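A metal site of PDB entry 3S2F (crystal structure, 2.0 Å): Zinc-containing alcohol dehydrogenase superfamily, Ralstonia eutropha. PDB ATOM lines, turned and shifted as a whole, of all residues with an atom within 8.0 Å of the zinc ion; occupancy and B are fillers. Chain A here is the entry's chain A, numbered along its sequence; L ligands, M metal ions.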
ATOM      1  N   GLY A  38     -14.724 -27.675 -33.013  1.00  0.00           N
ATOM      2  CA  GLY A  38     -13.985 -26.858 -32.080  1.00  0.00           C
ATOM      3  C   GLY A  38     -12.489 -26.779 -32.345  1.00  0.00           C
ATOM      4  O   GLY A  38     -11.866 -27.727 -32.807  1.00  0.00           O
ATOM      5  N   VAL A  39     -11.914 -25.617 -32.044  1.00  0.00           N
ATOM      6  CA  VAL A  39     -10.481 -25.391 -32.189  1.00  0.00           C
ATOM      7  C   VAL A  39      -9.864 -25.153 -30.810  1.00  0.00           C
ATOM      8  O   VAL A  39     -10.497 -24.533 -29.948  1.00  0.00           O
ATOM      9  CB  VAL A  39     -10.188 -24.173 -33.075  1.00  0.00           C
ATOM     10  CG1 VAL A  39      -8.693 -23.945 -33.205  1.00  0.00           C
ATOM     11  CG2 VAL A  39     -10.846 -24.328 -34.446  1.00  0.00           C
ATOM     12  N   CYS A  40      -8.646 -25.641 -30.596  1.00  0.00           N
ATOM     13  CA  CYS A  40      -7.951 -25.407 -29.341  1.00  0.00           C
ATOM     14  C   CYS A  40      -6.447 -25.550 -29.519  1.00  0.00           C
ATOM     15  O   CYS A  40      -5.972 -25.936 -30.597  1.00  0.00           O
ATOM     16  CB  CYS A  40      -8.428 -26.383 -28.262  1.00  0.00           C
ATOM     17  SG  CYS A  40      -7.540 -27.954 -28.239  1.00  0.00           S
ATOM     18  N   HIS A  41      -5.698 -25.251 -28.460  1.00  0.00           N
ATOM     19  CA  HIS A  41      -4.245 -25.272 -28.501  1.00  0.00           C
ATOM     20  C   HIS A  41      -3.639 -26.613 -28.932  1.00  0.00           C
ATOM     21  O   HIS A  41      -2.564 -26.645 -29.524  1.00  0.00           O
ATOM     22  CB  HIS A  41      -3.668 -24.831 -27.154  1.00  0.00           C
ATOM     23  CG  HIS A  41      -3.649 -23.344 -26.957  1.00  0.00           C
ATOM     24  ND1 HIS A  41      -2.538 -22.581 -27.218  1.00  0.00           N
ATOM     25  CD2 HIS A  41      -4.607 -22.486 -26.527  1.00  0.00           C
ATOM     26  CE1 HIS A  41      -2.799 -21.309 -26.959  1.00  0.00           C
ATOM     27  NE2 HIS A  41      -4.048 -21.229 -26.541  1.00  0.00           N
ATOM     28  N   THR A  42      -4.338 -27.711 -28.651  1.00  0.00           N
ATOM     29  CA  THR A  42      -3.854 -29.030 -29.029  1.00  0.00           C
ATOM     30  C   THR A  42      -3.688 -29.138 -30.542  1.00  0.00           C
ATOM     31  O   THR A  42      -2.791 -29.827 -31.043  1.00  0.00           O
ATOM     32  CB  THR A  42      -4.797 -30.143 -28.534  1.00  0.00           C
ATOM     33  OG1 THR A  42      -4.670 -30.270 -27.111  1.00  0.00           O
ATOM     34  CG2 THR A  42      -4.463 -31.471 -29.192  1.00  0.00           C
ATOM     35  N   ASP A  43      -4.563 -28.447 -31.274  1.00  0.00           N
ATOM     36  CA  ASP A  43      -4.509 -28.447 -32.730  1.00  0.00           C
ATOM     37  C   ASP A  43      -3.234 -27.775 -33.230  1.00  0.00           C
ATOM     38  O   ASP A  43      -2.703 -28.132 -34.281  1.00  0.00           O
ATOM     39  CB  ASP A  43      -5.737 -27.747 -33.310  1.00  0.00           C
ATOM     40  CG  ASP A  43      -7.028 -28.472 -32.969  1.00  0.00           C
ATOM     41  OD1 ASP A  43      -6.982 -29.715 -32.844  1.00  0.00           O
ATOM     42  OD2 ASP A  43      -8.072 -27.804 -32.812  1.00  0.00           O
ATOM     43  N   GLY A  62      -8.445 -31.724 -35.770  1.00  0.00           N
ATOM     44  CA  GLY A  62      -9.788 -31.577 -35.243  1.00  0.00           C
ATOM     45  C   GLY A  62     -10.268 -32.756 -34.423  1.00  0.00           C
ATOM     46  O   GLY A  62     -10.608 -33.803 -34.984  1.00  0.00           O
ATOM     47  N   HIS A  63     -10.309 -32.593 -33.109  1.00  0.00           N
ATOM     48  CA  HIS A  63     -10.801 -33.629 -32.212  1.00  0.00           C
ATOM     49  C   HIS A  63     -12.056 -33.159 -31.497  1.00  0.00           C
ATOM     50  O   HIS A  63     -12.472 -33.732 -30.493  1.00  0.00           O
ATOM     51  CB  HIS A  63      -9.723 -33.987 -31.176  1.00  0.00           C
ATOM     52  CG  HIS A  63      -9.173 -32.800 -30.454  1.00  0.00           C
ATOM     53  ND1 HIS A  63      -8.163 -32.020 -30.962  1.00  0.00           N
ATOM     54  CD2 HIS A  63      -9.506 -32.270 -29.251  1.00  0.00           C
ATOM     55  CE1 HIS A  63      -7.890 -31.048 -30.095  1.00  0.00           C
ATOM     56  NE2 HIS A  63      -8.673 -31.176 -29.057  1.00  0.00           N
ATOM     57  N   GLU A  64     -12.679 -32.107 -32.024  1.00  0.00           N
ATOM     58  CA  GLU A  64     -13.875 -31.531 -31.429  1.00  0.00           C
ATOM     59  C   GLU A  64     -14.990 -31.385 -32.453  1.00  0.00           C
ATOM     60  O   GLU A  64     -15.817 -30.464 -32.361  1.00  0.00           O
ATOM     61  CB  GLU A  64     -13.569 -30.175 -30.808  1.00  0.00           C
ATOM     62  CG  GLU A  64     -12.484 -30.170 -29.748  1.00  0.00           C
ATOM     63  CD  GLU A  64     -12.268 -28.797 -29.165  1.00  0.00           C
ATOM     64  OE1 GLU A  64     -13.196 -27.958 -29.243  1.00  0.00           O
ATOM     65  OE2 GLU A  64     -11.171 -28.532 -28.630  1.00  0.00           O
ATOM     66  N   TRP A  89     -11.212 -36.672 -28.923  1.00  0.00           N
ATOM     67  CA  TRP A  89      -9.805 -37.064 -28.881  1.00  0.00           C
ATOM     68  C   TRP A  89      -9.576 -38.574 -28.951  1.00  0.00           C
ATOM     69  O   TRP A  89      -8.763 -39.044 -29.745  1.00  0.00           O
ATOM     70  CB  TRP A  89      -9.146 -36.465 -27.638  1.00  0.00           C
ATOM     71  CG  TRP A  89      -7.695 -36.813 -27.440  1.00  0.00           C
ATOM     72  CD1 TRP A  89      -7.176 -37.642 -26.484  1.00  0.00           C
ATOM     73  CD2 TRP A  89      -6.579 -36.346 -28.213  1.00  0.00           C
ATOM     74  NE1 TRP A  89      -5.813 -37.717 -26.601  1.00  0.00           N
ATOM     75  CE2 TRP A  89      -5.415 -36.936 -27.660  1.00  0.00           C
ATOM     76  CE3 TRP A  89      -6.445 -35.497 -29.310  1.00  0.00           C
ATOM     77  CZ2 TRP A  89      -4.143 -36.689 -28.170  1.00  0.00           C
ATOM     78  CZ3 TRP A  89      -5.173 -35.259 -29.810  1.00  0.00           C
ATOM     79  CH2 TRP A  89      -4.039 -35.856 -29.246  1.00  0.00           C
ATOM     80  N   TYR A 122     -11.674 -31.228 -39.033  1.00  0.00           N
ATOM     81  CA  TYR A 122     -11.456 -30.035 -39.854  1.00  0.00           C
ATOM     82  C   TYR A 122     -11.872 -30.293 -41.305  1.00  0.00           C
ATOM     83  O   TYR A 122     -11.230 -29.818 -42.234  1.00  0.00           O
ATOM     84  CB  TYR A 122      -9.981 -29.598 -39.830  1.00  0.00           C
ATOM     85  CG  TYR A 122      -9.555 -28.818 -38.607  1.00  0.00           C
ATOM     86  CD1 TYR A 122      -8.412 -28.027 -38.628  1.00  0.00           C
ATOM     87  CD2 TYR A 122     -10.292 -28.869 -37.424  1.00  0.00           C
ATOM     88  CE1 TYR A 122      -8.011 -27.321 -37.519  1.00  0.00           C
ATOM     89  CE2 TYR A 122      -9.892 -28.156 -36.310  1.00  0.00           C
ATOM     90  CZ  TYR A 122      -8.748 -27.380 -36.360  1.00  0.00           C
ATOM     91  OH  TYR A 122      -8.340 -26.670 -35.257  1.00  0.00           O
ATOM     92  N   ALA A 146     -19.682 -28.305 -28.985  1.00  0.00           N
ATOM     93  CA  ALA A 146     -18.401 -28.782 -29.496  1.00  0.00           C
ATOM     94  C   ALA A 146     -17.260 -28.811 -28.459  1.00  0.00           C
ATOM     95  O   ALA A 146     -16.591 -29.837 -28.304  1.00  0.00           O
ATOM     96  CB  ALA A 146     -17.987 -27.988 -30.733  1.00  0.00           C
ATOM     97  N   PRO A 147     -17.030 -27.689 -27.766  1.00  0.00           N
ATOM     98  CA  PRO A 147     -15.918 -27.619 -26.806  1.00  0.00           C
ATOM     99  C   PRO A 147     -16.058 -28.571 -25.628  1.00  0.00           C
ATOM    100  O   PRO A 147     -15.059 -28.858 -24.957  1.00  0.00           O
ATOM    101  CB  PRO A 147     -15.963 -26.166 -26.324  1.00  0.00           C
ATOM    102  CG  PRO A 147     -16.656 -25.434 -27.415  1.00  0.00           C
ATOM    103  CD  PRO A 147     -17.688 -26.385 -27.935  1.00  0.00           C
ATOM    104  N   LEU A 149     -16.558 -31.611 -25.741  1.00  0.00           N
ATOM    105  CA  LEU A 149     -15.835 -32.811 -26.124  1.00  0.00           C
ATOM    106  C   LEU A 149     -14.381 -32.764 -25.669  1.00  0.00           C
ATOM    107  O   LEU A 149     -13.715 -33.790 -25.596  1.00  0.00           O
ATOM    108  CB  LEU A 149     -15.878 -33.005 -27.641  1.00  0.00           C
ATOM    109  CG  LEU A 149     -17.226 -33.303 -28.311  1.00  0.00           C
ATOM    110  CD1 LEU A 149     -17.063 -33.308 -29.826  1.00  0.00           C
ATOM    111  CD2 LEU A 149     -17.767 -34.643 -27.820  1.00  0.00           C
ATOM    112  N   CYS A 150     -13.895 -31.560 -25.389  1.00  0.00           N
ATOM    113  CA  CYS A 150     -12.497 -31.381 -25.005  1.00  0.00           C
ATOM    114  C   CYS A 150     -12.334 -30.687 -23.672  1.00  0.00           C
ATOM    115  O   CYS A 150     -11.965 -31.308 -22.672  1.00  0.00           O
ATOM    116  CB  CYS A 150     -11.751 -30.591 -26.075  1.00  0.00           C
ATOM    117  SG  CYS A 150     -10.050 -30.197 -25.609  1.00  0.00           S
ATOM    118  N   ALA A 151     -12.575 -29.374 -23.658  1.00  0.00           N
ATOM    119  CA  ALA A 151     -12.439 -28.587 -22.443  1.00  0.00           C
ATOM    120  C   ALA A 151     -13.387 -29.115 -21.381  1.00  0.00           C
ATOM    121  O   ALA A 151     -13.009 -29.311 -20.227  1.00  0.00           O
ATOM    122  CB  ALA A 151     -12.745 -27.133 -22.738  1.00  0.00           C
ATOM    123  N   THR A 154     -12.480 -32.622 -19.997  1.00  0.00           N
ATOM    124  CA  THR A 154     -11.164 -32.484 -19.382  1.00  0.00           C
ATOM    125  C   THR A 154     -11.238 -31.933 -17.963  1.00  0.00           C
ATOM    126  O   THR A 154     -10.717 -32.545 -17.025  1.00  0.00           O
ATOM    127  CB  THR A 154     -10.221 -31.612 -20.218  1.00  0.00           C
ATOM    128  OG1 THR A 154      -9.738 -32.369 -21.327  1.00  0.00           O
ATOM    129  CG2 THR A 154      -9.031 -31.146 -19.373  1.00  0.00           C
ATOM    130  N   LEU A 178      -9.916 -23.437 -20.535  1.00  0.00           N
ATOM    131  CA  LEU A 178     -10.407 -24.534 -19.705  1.00  0.00           C
ATOM    132  C   LEU A 178     -11.071 -24.020 -18.433  1.00  0.00           C
ATOM    133  O   LEU A 178     -12.160 -24.463 -18.062  1.00  0.00           O
ATOM    134  CB  LEU A 178      -9.264 -25.467 -19.315  1.00  0.00           C
ATOM    135  CG  LEU A 178      -8.557 -26.290 -20.404  1.00  0.00           C
ATOM    136  CD1 LEU A 178      -7.897 -27.493 -19.749  1.00  0.00           C
ATOM    137  CD2 LEU A 178      -9.538 -26.736 -21.469  1.00  0.00           C
ATOM    138  N   VAL A 288      -8.593 -34.985 -20.818  1.00  0.00           N
ATOM    139  CA  VAL A 288      -9.823 -35.575 -21.358  1.00  0.00           C
ATOM    140  C   VAL A 288     -10.424 -36.590 -20.391  1.00  0.00           C
ATOM    141  O   VAL A 288     -10.291 -36.453 -19.174  1.00  0.00           O
ATOM    142  CB  VAL A 288      -9.645 -36.175 -22.780  1.00  0.00           C
ATOM    143  CG1 VAL A 288      -9.128 -35.125 -23.744  1.00  0.00           C
ATOM    144  CG2 VAL A 288      -8.736 -37.391 -22.757  1.00  0.00           C
ATOM    145  N   ARG A 333     -13.566 -20.058 -26.394  1.00  0.00           N
ATOM    146  CA  ARG A 333     -13.203 -21.050 -27.399  1.00  0.00           C
ATOM    147  C   ARG A 333     -13.726 -20.661 -28.782  1.00  0.00           C
ATOM    148  O   ARG A 333     -14.850 -20.197 -28.917  1.00  0.00           O
ATOM    149  CB  ARG A 333     -13.748 -22.429 -27.020  1.00  0.00           C
ATOM    150  CG  ARG A 333     -12.873 -23.206 -26.050  1.00  0.00           C
ATOM    151  CD  ARG A 333     -11.600 -23.691 -26.712  1.00  0.00           C
ATOM    152  NE  ARG A 333     -10.824 -24.558 -25.838  1.00  0.00           N
ATOM    153  CZ  ARG A 333     -10.991 -25.874 -25.750  1.00  0.00           C
ATOM    154  NH1 ARG A 333     -10.235 -26.590 -24.922  1.00  0.00           N
ATOM    155  NH2 ARG A 333     -11.916 -26.482 -26.480  1.00  0.00           N
HETATM  156  C1  LIG L   1      -7.490 -33.375 -26.442  1.00  0.00           C
HETATM  157  C2  LIG L   1      -6.397 -32.816 -25.586  1.00  0.00           C
HETATM  158  C3  LIG L   1      -5.342 -33.863 -25.355  1.00  0.00           C
HETATM  159  O1  LIG L   1      -6.178 -31.605 -25.491  1.00  0.00           O
HETATM  160 ZN    ZN M   1      -9.440 -29.505 -27.946  1.00  0.00          ZN
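The side-chain hydroxyl (OG1) of Thr 42 sits at hydrogen-bond distance from an oxygen (O1) of the ligand (2.6 Å).
The guanidinium group of Arg 333 lies within salt-bridge range of the side-chain carboxylate of Glu 64 (3.4 Å).
The backbone carbonyl oxygen of Glu 64 sits at hydrogen-bond distance from the backbone NH of Gly 38.
The side-chain carboxylate of Asp 43 sits close to a ring nitrogen (ND1) of His 63 (3.2 Å).
The backbone NH (N) of Thr 42 lies close to the side-chain sulfur (SG) of Cys 40, at 3.2 Å.
The side-chain carboxylate (OD2) of Asp 43 lies within hydrogen-bond range of the backbone NH (N) of Cys 40 (3.1 Å).
The side-chain sulfur (SG) of Cys 150 lies close to the guanidinium group (NH1) of Arg 333 (3.7 Å).
OG1 of Thr 154 lies within hydrogen-bond range of O of Cys 150 (2.8 Å).
Of the 20 residues printed, 4 come within 4 Å of the zinc ion.
Along chain A the residues within 4 Å of the zinc ion span positions 40 to 150.
The zinc ion is bound by the side-chain carboxylate (OE2) of Glu 64 (2.1 Å), a ring nitrogen (NE2) of His 63 (2.1 Å), the side-chain sulfur (SG) of Cys 40 (2.5 Å) and the side-chain sulfur (SG) of Cys 150 (2.5 Å).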
